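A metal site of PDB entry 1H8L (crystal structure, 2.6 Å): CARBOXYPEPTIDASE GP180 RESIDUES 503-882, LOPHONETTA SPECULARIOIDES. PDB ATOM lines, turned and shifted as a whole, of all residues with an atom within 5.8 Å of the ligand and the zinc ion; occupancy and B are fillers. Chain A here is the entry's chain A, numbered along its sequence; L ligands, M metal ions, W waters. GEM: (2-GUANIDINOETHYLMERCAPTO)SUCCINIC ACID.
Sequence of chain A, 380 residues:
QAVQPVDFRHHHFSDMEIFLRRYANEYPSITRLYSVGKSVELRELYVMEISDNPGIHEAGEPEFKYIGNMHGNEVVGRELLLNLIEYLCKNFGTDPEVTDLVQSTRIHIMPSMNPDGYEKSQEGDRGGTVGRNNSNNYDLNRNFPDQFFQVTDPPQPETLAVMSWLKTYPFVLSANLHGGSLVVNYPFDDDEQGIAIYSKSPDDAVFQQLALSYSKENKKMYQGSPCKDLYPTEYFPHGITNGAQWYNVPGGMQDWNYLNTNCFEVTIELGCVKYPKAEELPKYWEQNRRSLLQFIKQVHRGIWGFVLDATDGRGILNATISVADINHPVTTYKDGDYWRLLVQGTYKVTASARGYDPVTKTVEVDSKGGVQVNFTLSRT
The side-chain amide oxygen (OD1) of Asn 185 sits close to a nitrogen (N3) of the ligand (3.4 Å). The guanidinium group (NH2) of Arg 142 lies within salt-bridge range of an oxygen (O15) of the ligand. O of Tyr 247 is in hydrogen-bond range of N4 of the ligand (2.5 Å). The side-chain carboxylate (OD1) of Asp 189 lies within salt-bridge range of a nitrogen (N2) of the ligand (2.5 Å). An oxygen (O14) of the ligand lies within salt-bridge range of the guanidinium group (NH2) of Arg 132 (2.7 Å). O15 of the ligand lies within hydrogen-bond range of ND2 of Asn 141, at 2.9 Å. The backbone carbonyl oxygen of Gly 243 is in hydrogen-bond range of a nitrogen (N4) of the ligand (3.2 Å).
OE1 of Glu 74 sits close to NH1 of Arg 132, 3.4 Å away. The side-chain carboxylate (OD2) of Asp 139 lies within salt-bridge range of the guanidinium group (NH2) of Arg 142, at 3.9 Å. The side-chain carboxylate (OD1) of Asp 189 lies within hydrogen-bond range of the side-chain amide nitrogen (ND2) of Asn 185 (2.9 Å). The backbone carbonyl oxygen (O) of Asn 185 lies close to the side-chain amide oxygen (OE1) of Gln 254 (3.0 Å). The backbone carbonyl oxygen (O) of Asp 189 is in hydrogen-bond range of the backbone NH (N) of Val 249, 2.8 Å away. N of Asn 185 lies within hydrogen-bond range of O of Thr 267 (2.6 Å). The side-chain carboxylate (OE2) of Glu 74 sits close to the backbone NH (N) of Gly 179 (3.0 Å). The side-chain carboxylate (OE2) of Glu 269 sits close to the backbone NH (N) of Gly 179 (3.5 Å).
O of Gly 179 sits close to O13 of the ligand, 3.5 Å away. The side-chain carboxylate (OE1) of Glu 269 sits close to an oxygen (O13) of the ligand, at 2.9 Å. Residues that only touch the ligand: Val 249 and Trp 246. Hydrophobic or aromatic side chains within 4 Å of the ligand: His 71, His 178, Trp 246, Tyr 247 and Val 249. Of the 24 residues printed, 14 come within 4 Å of the ligand.
Three residues have an atom within 4 Å of the zinc ion: His 71, Glu 74 and His 178. The nearest printed residue that does not touch the zinc ion is Arg 132 (4.04 Å).
The zinc ion is bound by ND1 of His 178 (2.0 Å), ND1 of His 71 (2.0 Å), OE2 of Glu 74 (2.1 Å), O12 of the ligand (2.2 Å), O13 of the ligand (2.2 Å) and OE1 of Glu 74 (2.6 Å). The zinc ion has six donor atoms within binding distance.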
ATOM      1  N   HIS A  71     -24.846 -18.745  -7.782  1.00  0.00           N
ATOM      2  CA  HIS A  71     -24.830 -18.754  -9.225  1.00  0.00           C
ATOM      3  C   HIS A  71     -26.234 -18.303  -9.600  1.00  0.00           C
ATOM      4  O   HIS A  71     -27.207 -19.011  -9.350  1.00  0.00           O
ATOM      5  CB  HIS A  71     -24.555 -20.168  -9.759  1.00  0.00           C
ATOM      6  CG  HIS A  71     -23.116 -20.585  -9.665  1.00  0.00           C
ATOM      7  ND1 HIS A  71     -22.755 -21.894  -9.486  1.00  0.00           N
ATOM      8  CD2 HIS A  71     -21.998 -19.816  -9.747  1.00  0.00           C
ATOM      9  CE1 HIS A  71     -21.440 -21.906  -9.474  1.00  0.00           C
ATOM     10  NE2 HIS A  71     -20.931 -20.674  -9.624  1.00  0.00           N
ATOM     11  N   GLU A  74     -29.162 -20.698 -10.810  1.00  0.00           N
ATOM     12  CA  GLU A  74     -29.451 -21.912 -10.035  1.00  0.00           C
ATOM     13  C   GLU A  74     -30.330 -21.377  -8.907  1.00  0.00           C
ATOM     14  O   GLU A  74     -29.878 -21.039  -7.820  1.00  0.00           O
ATOM     15  CB  GLU A  74     -28.147 -22.515  -9.530  1.00  0.00           C
ATOM     16  CG  GLU A  74     -27.244 -22.895 -10.697  1.00  0.00           C
ATOM     17  CD  GLU A  74     -25.869 -23.345 -10.272  1.00  0.00           C
ATOM     18  OE1 GLU A  74     -25.003 -23.502 -11.166  1.00  0.00           O
ATOM     19  OE2 GLU A  74     -25.644 -23.523  -9.055  1.00  0.00           O
ATOM     20  N   ARG A 132     -25.340 -16.894 -14.488  1.00  0.00           N
ATOM     21  CA  ARG A 132     -24.508 -17.646 -13.558  1.00  0.00           C
ATOM     22  C   ARG A 132     -23.471 -16.776 -12.852  1.00  0.00           C
ATOM     23  O   ARG A 132     -23.441 -16.728 -11.620  1.00  0.00           O
ATOM     24  CB  ARG A 132     -23.806 -18.781 -14.292  1.00  0.00           C
ATOM     25  CG  ARG A 132     -22.806 -19.540 -13.433  1.00  0.00           C
ATOM     26  CD  ARG A 132     -22.034 -20.510 -14.275  1.00  0.00           C
ATOM     27  NE  ARG A 132     -20.860 -21.056 -13.586  1.00  0.00           N
ATOM     28  CZ  ARG A 132     -20.865 -22.150 -12.829  1.00  0.00           C
ATOM     29  NH1 ARG A 132     -21.993 -22.842 -12.641  1.00  0.00           N
ATOM     30  NH2 ARG A 132     -19.737 -22.559 -12.248  1.00  0.00           N
ATOM     31  N   ASP A 139     -17.082 -15.798 -11.983  1.00  0.00           N
ATOM     32  CA  ASP A 139     -17.738 -16.882 -11.272  1.00  0.00           C
ATOM     33  C   ASP A 139     -17.413 -16.725  -9.784  1.00  0.00           C
ATOM     34  O   ASP A 139     -16.257 -16.869  -9.372  1.00  0.00           O
ATOM     35  CB  ASP A 139     -17.215 -18.229 -11.752  1.00  0.00           C
ATOM     36  CG  ASP A 139     -18.071 -19.389 -11.293  1.00  0.00           C
ATOM     37  OD1 ASP A 139     -18.506 -19.384 -10.126  1.00  0.00           O
ATOM     38  OD2 ASP A 139     -18.302 -20.319 -12.108  1.00  0.00           O
ATOM     39  N   ASN A 141     -17.943 -18.669  -7.505  1.00  0.00           N
ATOM     40  CA  ASN A 141     -17.469 -19.920  -6.929  1.00  0.00           C
ATOM     41  C   ASN A 141     -16.120 -20.342  -7.520  1.00  0.00           C
ATOM     42  O   ASN A 141     -15.771 -21.515  -7.546  1.00  0.00           O
ATOM     43  CB  ASN A 141     -18.505 -21.028  -7.097  1.00  0.00           C
ATOM     44  CG  ASN A 141     -18.301 -22.181  -6.123  1.00  0.00           C
ATOM     45  OD1 ASN A 141     -17.994 -21.972  -4.943  1.00  0.00           O
ATOM     46  ND2 ASN A 141     -18.477 -23.396  -6.605  1.00  0.00           N
ATOM     47  N   ARG A 142     -15.374 -19.349  -7.999  1.00  0.00           N
ATOM     48  CA  ARG A 142     -14.034 -19.515  -8.552  1.00  0.00           C
ATOM     49  C   ARG A 142     -13.261 -18.327  -8.000  1.00  0.00           C
ATOM     50  O   ARG A 142     -12.056 -18.195  -8.206  1.00  0.00           O
ATOM     51  CB  ARG A 142     -14.034 -19.401 -10.071  1.00  0.00           C
ATOM     52  CG  ARG A 142     -14.771 -20.483 -10.779  1.00  0.00           C
ATOM     53  CD  ARG A 142     -14.041 -21.811 -10.636  1.00  0.00           C
ATOM     54  NE  ARG A 142     -14.753 -22.864 -11.345  1.00  0.00           N
ATOM     55  CZ  ARG A 142     -15.912 -23.370 -10.946  1.00  0.00           C
ATOM     56  NH1 ARG A 142     -16.503 -24.319 -11.655  1.00  0.00           N
ATOM     57  NH2 ARG A 142     -16.463 -22.952  -9.818  1.00  0.00           N
ATOM     58  N   LEU A 177     -26.203 -23.676  -1.434  1.00  0.00           N
ATOM     59  CA  LEU A 177     -27.010 -24.394  -2.418  1.00  0.00           C
ATOM     60  C   LEU A 177     -26.816 -24.055  -3.886  1.00  0.00           C
ATOM     61  O   LEU A 177     -26.709 -22.898  -4.265  1.00  0.00           O
ATOM     62  CB  LEU A 177     -28.476 -24.228  -2.041  1.00  0.00           C
ATOM     63  CG  LEU A 177     -28.720 -24.283  -0.535  1.00  0.00           C
ATOM     64  CD1 LEU A 177     -30.178 -24.048  -0.225  1.00  0.00           C
ATOM     65  CD2 LEU A 177     -28.290 -25.632   0.000  1.00  0.00           C
ATOM     66  N   HIS A 178     -26.818 -25.105  -4.711  1.00  0.00           N
ATOM     67  CA  HIS A 178     -26.655 -24.972  -6.158  1.00  0.00           C
ATOM     68  C   HIS A 178     -27.672 -25.806  -6.932  1.00  0.00           C
ATOM     69  O   HIS A 178     -28.519 -26.495  -6.352  1.00  0.00           O
ATOM     70  CB  HIS A 178     -25.261 -25.442  -6.586  1.00  0.00           C
ATOM     71  CG  HIS A 178     -24.157 -24.547  -6.144  1.00  0.00           C
ATOM     72  ND1 HIS A 178     -23.448 -23.780  -7.033  1.00  0.00           N
ATOM     73  CD2 HIS A 178     -23.675 -24.339  -4.884  1.00  0.00           C
ATOM     74  CE1 HIS A 178     -22.551 -23.138  -6.316  1.00  0.00           C
ATOM     75  NE2 HIS A 178     -22.648 -23.434  -5.009  1.00  0.00           N
ATOM     76  N   GLY A 179     -27.562 -25.743  -8.247  1.00  0.00           N
ATOM     77  CA  GLY A 179     -28.427 -26.480  -9.137  1.00  0.00           C
ATOM     78  C   GLY A 179     -27.601 -26.954 -10.318  1.00  0.00           C
ATOM     79  O   GLY A 179     -26.581 -26.347 -10.644  1.00  0.00           O
ATOM     80  N   GLY A 180     -28.032 -28.024 -10.952  1.00  0.00           N
ATOM     81  CA  GLY A 180     -27.286 -28.546 -12.091  1.00  0.00           C
ATOM     82  C   GLY A 180     -26.993 -30.012 -11.862  1.00  0.00           C
ATOM     83  O   GLY A 180     -26.370 -30.659 -12.702  1.00  0.00           O
ATOM     84  N   ASN A 185     -22.189 -32.336  -2.139  1.00  0.00           N
ATOM     85  CA  ASN A 185     -20.759 -32.235  -2.431  1.00  0.00           C
ATOM     86  C   ASN A 185     -19.943 -31.808  -1.195  1.00  0.00           C
ATOM     87  O   ASN A 185     -20.295 -30.823  -0.536  1.00  0.00           O
ATOM     88  CB  ASN A 185     -20.635 -31.195  -3.554  1.00  0.00           C
ATOM     89  CG  ASN A 185     -19.226 -30.988  -4.047  1.00  0.00           C
ATOM     90  OD1 ASN A 185     -18.812 -31.619  -5.023  1.00  0.00           O
ATOM     91  ND2 ASN A 185     -18.488 -30.105  -3.402  1.00  0.00           N
ATOM     92  N   PHE A 188     -12.315 -32.016  -0.210  1.00  0.00           N
ATOM     93  CA  PHE A 188     -11.927 -30.805  -0.935  1.00  0.00           C
ATOM     94  C   PHE A 188     -12.490 -30.766  -2.361  1.00  0.00           C
ATOM     95  O   PHE A 188     -12.753 -31.818  -2.952  1.00  0.00           O
ATOM     96  CB  PHE A 188     -10.406 -30.718  -1.018  1.00  0.00           C
ATOM     97  CG  PHE A 188      -9.743 -30.479   0.296  1.00  0.00           C
ATOM     98  CD1 PHE A 188     -10.137 -29.409   1.099  1.00  0.00           C
ATOM     99  CD2 PHE A 188      -8.715 -31.297   0.720  1.00  0.00           C
ATOM    100  CE1 PHE A 188      -9.494 -29.157   2.305  1.00  0.00           C
ATOM    101  CE2 PHE A 188      -8.058 -31.060   1.919  1.00  0.00           C
ATOM    102  CZ  PHE A 188      -8.452 -29.990   2.722  1.00  0.00           C
ATOM    103  N   ASP A 189     -12.656 -29.552  -2.903  1.00  0.00           N
ATOM    104  CA  ASP A 189     -13.199 -29.362  -4.244  1.00  0.00           C
ATOM    105  C   ASP A 189     -12.171 -29.474  -5.354  1.00  0.00           C
ATOM    106  O   ASP A 189     -12.520 -29.569  -6.532  1.00  0.00           O
ATOM    107  CB  ASP A 189     -13.855 -27.987  -4.383  1.00  0.00           C
ATOM    108  CG  ASP A 189     -15.312 -28.009  -4.011  1.00  0.00           C
ATOM    109  OD1 ASP A 189     -15.968 -29.038  -4.239  1.00  0.00           O
ATOM    110  OD2 ASP A 189     -15.795 -26.974  -3.511  1.00  0.00           O
ATOM    111  N   ASP A 190     -10.897 -29.455  -4.983  1.00  0.00           N
ATOM    112  CA  ASP A 190      -9.841 -29.545  -5.976  1.00  0.00           C
ATOM    113  C   ASP A 190      -8.621 -30.201  -5.359  1.00  0.00           C
ATOM    114  O   ASP A 190      -8.587 -30.484  -4.166  1.00  0.00           O
ATOM    115  CB  ASP A 190      -9.516 -28.153  -6.514  1.00  0.00           C
ATOM    116  CG  ASP A 190      -8.816 -27.265  -5.490  1.00  0.00           C
ATOM    117  OD1 ASP A 190      -9.054 -27.405  -4.272  1.00  0.00           O
ATOM    118  OD2 ASP A 190      -8.021 -26.414  -5.928  1.00  0.00           O
ATOM    119  N   ASN A 242     -17.314 -36.427  -3.141  1.00  0.00           N
ATOM    120  CA  ASN A 242     -16.191 -35.578  -2.809  1.00  0.00           C
ATOM    121  C   ASN A 242     -16.149 -34.619  -3.999  1.00  0.00           C
ATOM    122  O   ASN A 242     -16.334 -35.044  -5.136  1.00  0.00           O
ATOM    123  CB  ASN A 242     -14.913 -36.413  -2.696  1.00  0.00           C
ATOM    124  CG  ASN A 242     -13.639 -35.578  -2.781  1.00  0.00           C
ATOM    125  OD1 ASN A 242     -12.966 -35.576  -3.801  1.00  0.00           O
ATOM    126  ND2 ASN A 242     -13.312 -34.878  -1.697  1.00  0.00           N
ATOM    127  N   GLY A 243     -15.930 -33.335  -3.733  1.00  0.00           N
ATOM    128  CA  GLY A 243     -15.903 -32.375  -4.817  1.00  0.00           C
ATOM    129  C   GLY A 243     -14.955 -32.745  -5.944  1.00  0.00           C
ATOM    130  O   GLY A 243     -15.366 -33.007  -7.074  1.00  0.00           O
ATOM    131  N   ALA A 244     -13.663 -32.757  -5.619  1.00  0.00           N
ATOM    132  CA  ALA A 244     -12.605 -33.062  -6.576  1.00  0.00           C
ATOM    133  C   ALA A 244     -12.849 -34.310  -7.406  1.00  0.00           C
ATOM    134  O   ALA A 244     -12.553 -34.321  -8.602  1.00  0.00           O
ATOM    135  CB  ALA A 244     -11.275 -33.182  -5.862  1.00  0.00           C
ATOM    136  N   TRP A 246     -15.620 -35.604  -8.367  1.00  0.00           N
ATOM    137  CA  TRP A 246     -16.633 -35.338  -9.375  1.00  0.00           C
ATOM    138  C   TRP A 246     -15.866 -34.591 -10.481  1.00  0.00           C
ATOM    139  O   TRP A 246     -15.888 -34.996 -11.654  1.00  0.00           O
ATOM    140  CB  TRP A 246     -17.732 -34.483  -8.761  1.00  0.00           C
ATOM    141  CG  TRP A 246     -18.844 -34.210  -9.675  1.00  0.00           C
ATOM    142  CD1 TRP A 246     -19.037 -34.753 -10.918  1.00  0.00           C
ATOM    143  CD2 TRP A 246     -19.933 -33.300  -9.460  1.00  0.00           C
ATOM    144  NE1 TRP A 246     -20.181 -34.240 -11.490  1.00  0.00           N
ATOM    145  CE2 TRP A 246     -20.748 -33.336 -10.614  1.00  0.00           C
ATOM    146  CE3 TRP A 246     -20.287 -32.447  -8.400  1.00  0.00           C
ATOM    147  CZ2 TRP A 246     -21.906 -32.566 -10.740  1.00  0.00           C
ATOM    148  CZ3 TRP A 246     -21.439 -31.674  -8.519  1.00  0.00           C
ATOM    149  CH2 TRP A 246     -22.232 -31.738  -9.682  1.00  0.00           C
ATOM    150  N   TYR A 247     -15.198 -33.513 -10.103  1.00  0.00           N
ATOM    151  CA  TYR A 247     -14.357 -32.739 -11.011  1.00  0.00           C
ATOM    152  C   TYR A 247     -13.686 -31.591 -10.269  1.00  0.00           C
ATOM    153  O   TYR A 247     -14.242 -31.064  -9.302  1.00  0.00           O
ATOM    154  CB  TYR A 247     -15.138 -32.270 -12.249  1.00  0.00           C
ATOM    155  CG  TYR A 247     -16.229 -31.257 -12.022  1.00  0.00           C
ATOM    156  CD1 TYR A 247     -15.947 -29.887 -12.009  1.00  0.00           C
ATOM    157  CD2 TYR A 247     -17.564 -31.664 -11.892  1.00  0.00           C
ATOM    158  CE1 TYR A 247     -16.966 -28.952 -11.873  1.00  0.00           C
ATOM    159  CE2 TYR A 247     -18.584 -30.729 -11.756  1.00  0.00           C
ATOM    160  CZ  TYR A 247     -18.274 -29.376 -11.749  1.00  0.00           C
ATOM    161  OH  TYR A 247     -19.289 -28.443 -11.642  1.00  0.00           O
ATOM    162  N   ASN A 248     -12.486 -31.238 -10.684  1.00  0.00           N
ATOM    163  CA  ASN A 248     -11.708 -30.198 -10.039  1.00  0.00           C
ATOM    164  C   ASN A 248     -12.339 -28.800 -10.138  1.00  0.00           C
ATOM    165  O   ASN A 248     -12.705 -28.344 -11.224  1.00  0.00           O
ATOM    166  CB  ASN A 248     -10.292 -30.197 -10.637  1.00  0.00           C
ATOM    167  CG  ASN A 248      -9.302 -29.420  -9.797  1.00  0.00           C
ATOM    168  OD1 ASN A 248      -8.853 -29.890  -8.750  1.00  0.00           O
ATOM    169  ND2 ASN A 248      -8.953 -28.227 -10.257  1.00  0.00           N
ATOM    170  N   VAL A 249     -12.453 -28.148  -8.990  1.00  0.00           N
ATOM    171  CA  VAL A 249     -13.006 -26.793  -8.902  1.00  0.00           C
ATOM    172  C   VAL A 249     -12.162 -25.945  -7.961  1.00  0.00           C
ATOM    173  O   VAL A 249     -12.182 -26.162  -6.755  1.00  0.00           O
ATOM    174  CB  VAL A 249     -14.450 -26.777  -8.352  1.00  0.00           C
ATOM    175  CG1 VAL A 249     -14.871 -25.351  -8.046  1.00  0.00           C
ATOM    176  CG2 VAL A 249     -15.411 -27.386  -9.359  1.00  0.00           C
ATOM    177  N   GLN A 254     -16.788 -23.162  -0.623  1.00  0.00           N
ATOM    178  CA  GLN A 254     -16.854 -24.309   0.281  1.00  0.00           C
ATOM    179  C   GLN A 254     -15.549 -24.632   1.023  1.00  0.00           C
ATOM    180  O   GLN A 254     -15.546 -24.791   2.245  1.00  0.00           O
ATOM    181  CB  GLN A 254     -17.303 -25.535  -0.504  1.00  0.00           C
ATOM    182  CG  GLN A 254     -17.158 -26.818   0.264  1.00  0.00           C
ATOM    183  CD  GLN A 254     -17.389 -28.024  -0.591  1.00  0.00           C
ATOM    184  OE1 GLN A 254     -18.527 -28.387  -0.881  1.00  0.00           O
ATOM    185  NE2 GLN A 254     -16.315 -28.647  -1.013  1.00  0.00           N
ATOM    186  N   THR A 267     -21.562 -28.385  -0.062  1.00  0.00           N
ATOM    187  CA  THR A 267     -22.261 -27.805  -1.214  1.00  0.00           C
ATOM    188  C   THR A 267     -23.396 -28.726  -1.648  1.00  0.00           C
ATOM    189  O   THR A 267     -23.171 -29.891  -1.960  1.00  0.00           O
ATOM    190  CB  THR A 267     -21.315 -27.626  -2.409  1.00  0.00           C
ATOM    191  OG1 THR A 267     -20.170 -26.864  -2.015  1.00  0.00           O
ATOM    192  CG2 THR A 267     -22.016 -26.900  -3.521  1.00  0.00           C
ATOM    193  N   GLU A 269     -26.462 -29.767  -4.256  1.00  0.00           N
ATOM    194  CA  GLU A 269     -27.031 -29.648  -5.594  1.00  0.00           C
ATOM    195  C   GLU A 269     -28.465 -30.145  -5.475  1.00  0.00           C
ATOM    196  O   GLU A 269     -28.701 -31.331  -5.260  1.00  0.00           O
ATOM    197  CB  GLU A 269     -26.232 -30.504  -6.573  1.00  0.00           C
ATOM    198  CG  GLU A 269     -24.782 -30.057  -6.730  1.00  0.00           C
ATOM    199  CD  GLU A 269     -24.610 -28.935  -7.742  1.00  0.00           C
ATOM    200  OE1 GLU A 269     -23.489 -28.386  -7.855  1.00  0.00           O
ATOM    201  OE2 GLU A 269     -25.600 -28.608  -8.428  1.00  0.00           O
HETATM  202  C8  GEM L   1     -19.914 -26.489  -9.208  1.00  0.00           C
HETATM  203  S7  GEM L   1     -19.813 -26.350  -7.406  1.00  0.00           S
HETATM  204  C6  GEM L   1     -20.161 -28.038  -6.908  1.00  0.00           C
HETATM  205  C5  GEM L   1     -18.878 -28.749  -6.515  1.00  0.00           C
HETATM  206  N3  GEM L   1     -18.285 -29.460  -7.631  1.00  0.00           N
HETATM  207  C1  GEM L   1     -17.006 -29.825  -7.700  1.00  0.00           C
HETATM  208  N4  GEM L   1     -16.564 -30.497  -8.741  1.00  0.00           N
HETATM  209  N2  GEM L   1     -16.172 -29.530  -6.706  1.00  0.00           N
HETATM  210  C9  GEM L   1     -19.392 -25.208  -9.878  1.00  0.00           C
HETATM  211  O14 GEM L   1     -19.891 -24.896 -10.957  1.00  0.00           O
HETATM  212  O15 GEM L   1     -18.534 -24.516  -9.317  1.00  0.00           O
HETATM  213  C10 GEM L   1     -21.317 -26.828  -9.737  1.00  0.00           C
HETATM  214  C11 GEM L   1     -22.272 -25.663  -9.683  1.00  0.00           C
HETATM  215  O12 GEM L   1     -21.959 -24.557 -10.180  1.00  0.00           O
HETATM  216  O13 GEM L   1     -23.407 -25.892  -9.266  1.00  0.00           O
HETATM  217 ZN    ZN M   1     -23.576 -23.665  -9.021  1.00  0.00          ZN
HETATM  218  O   HOH W   1     -23.839 -26.065 -12.492  1.00  0.00           O
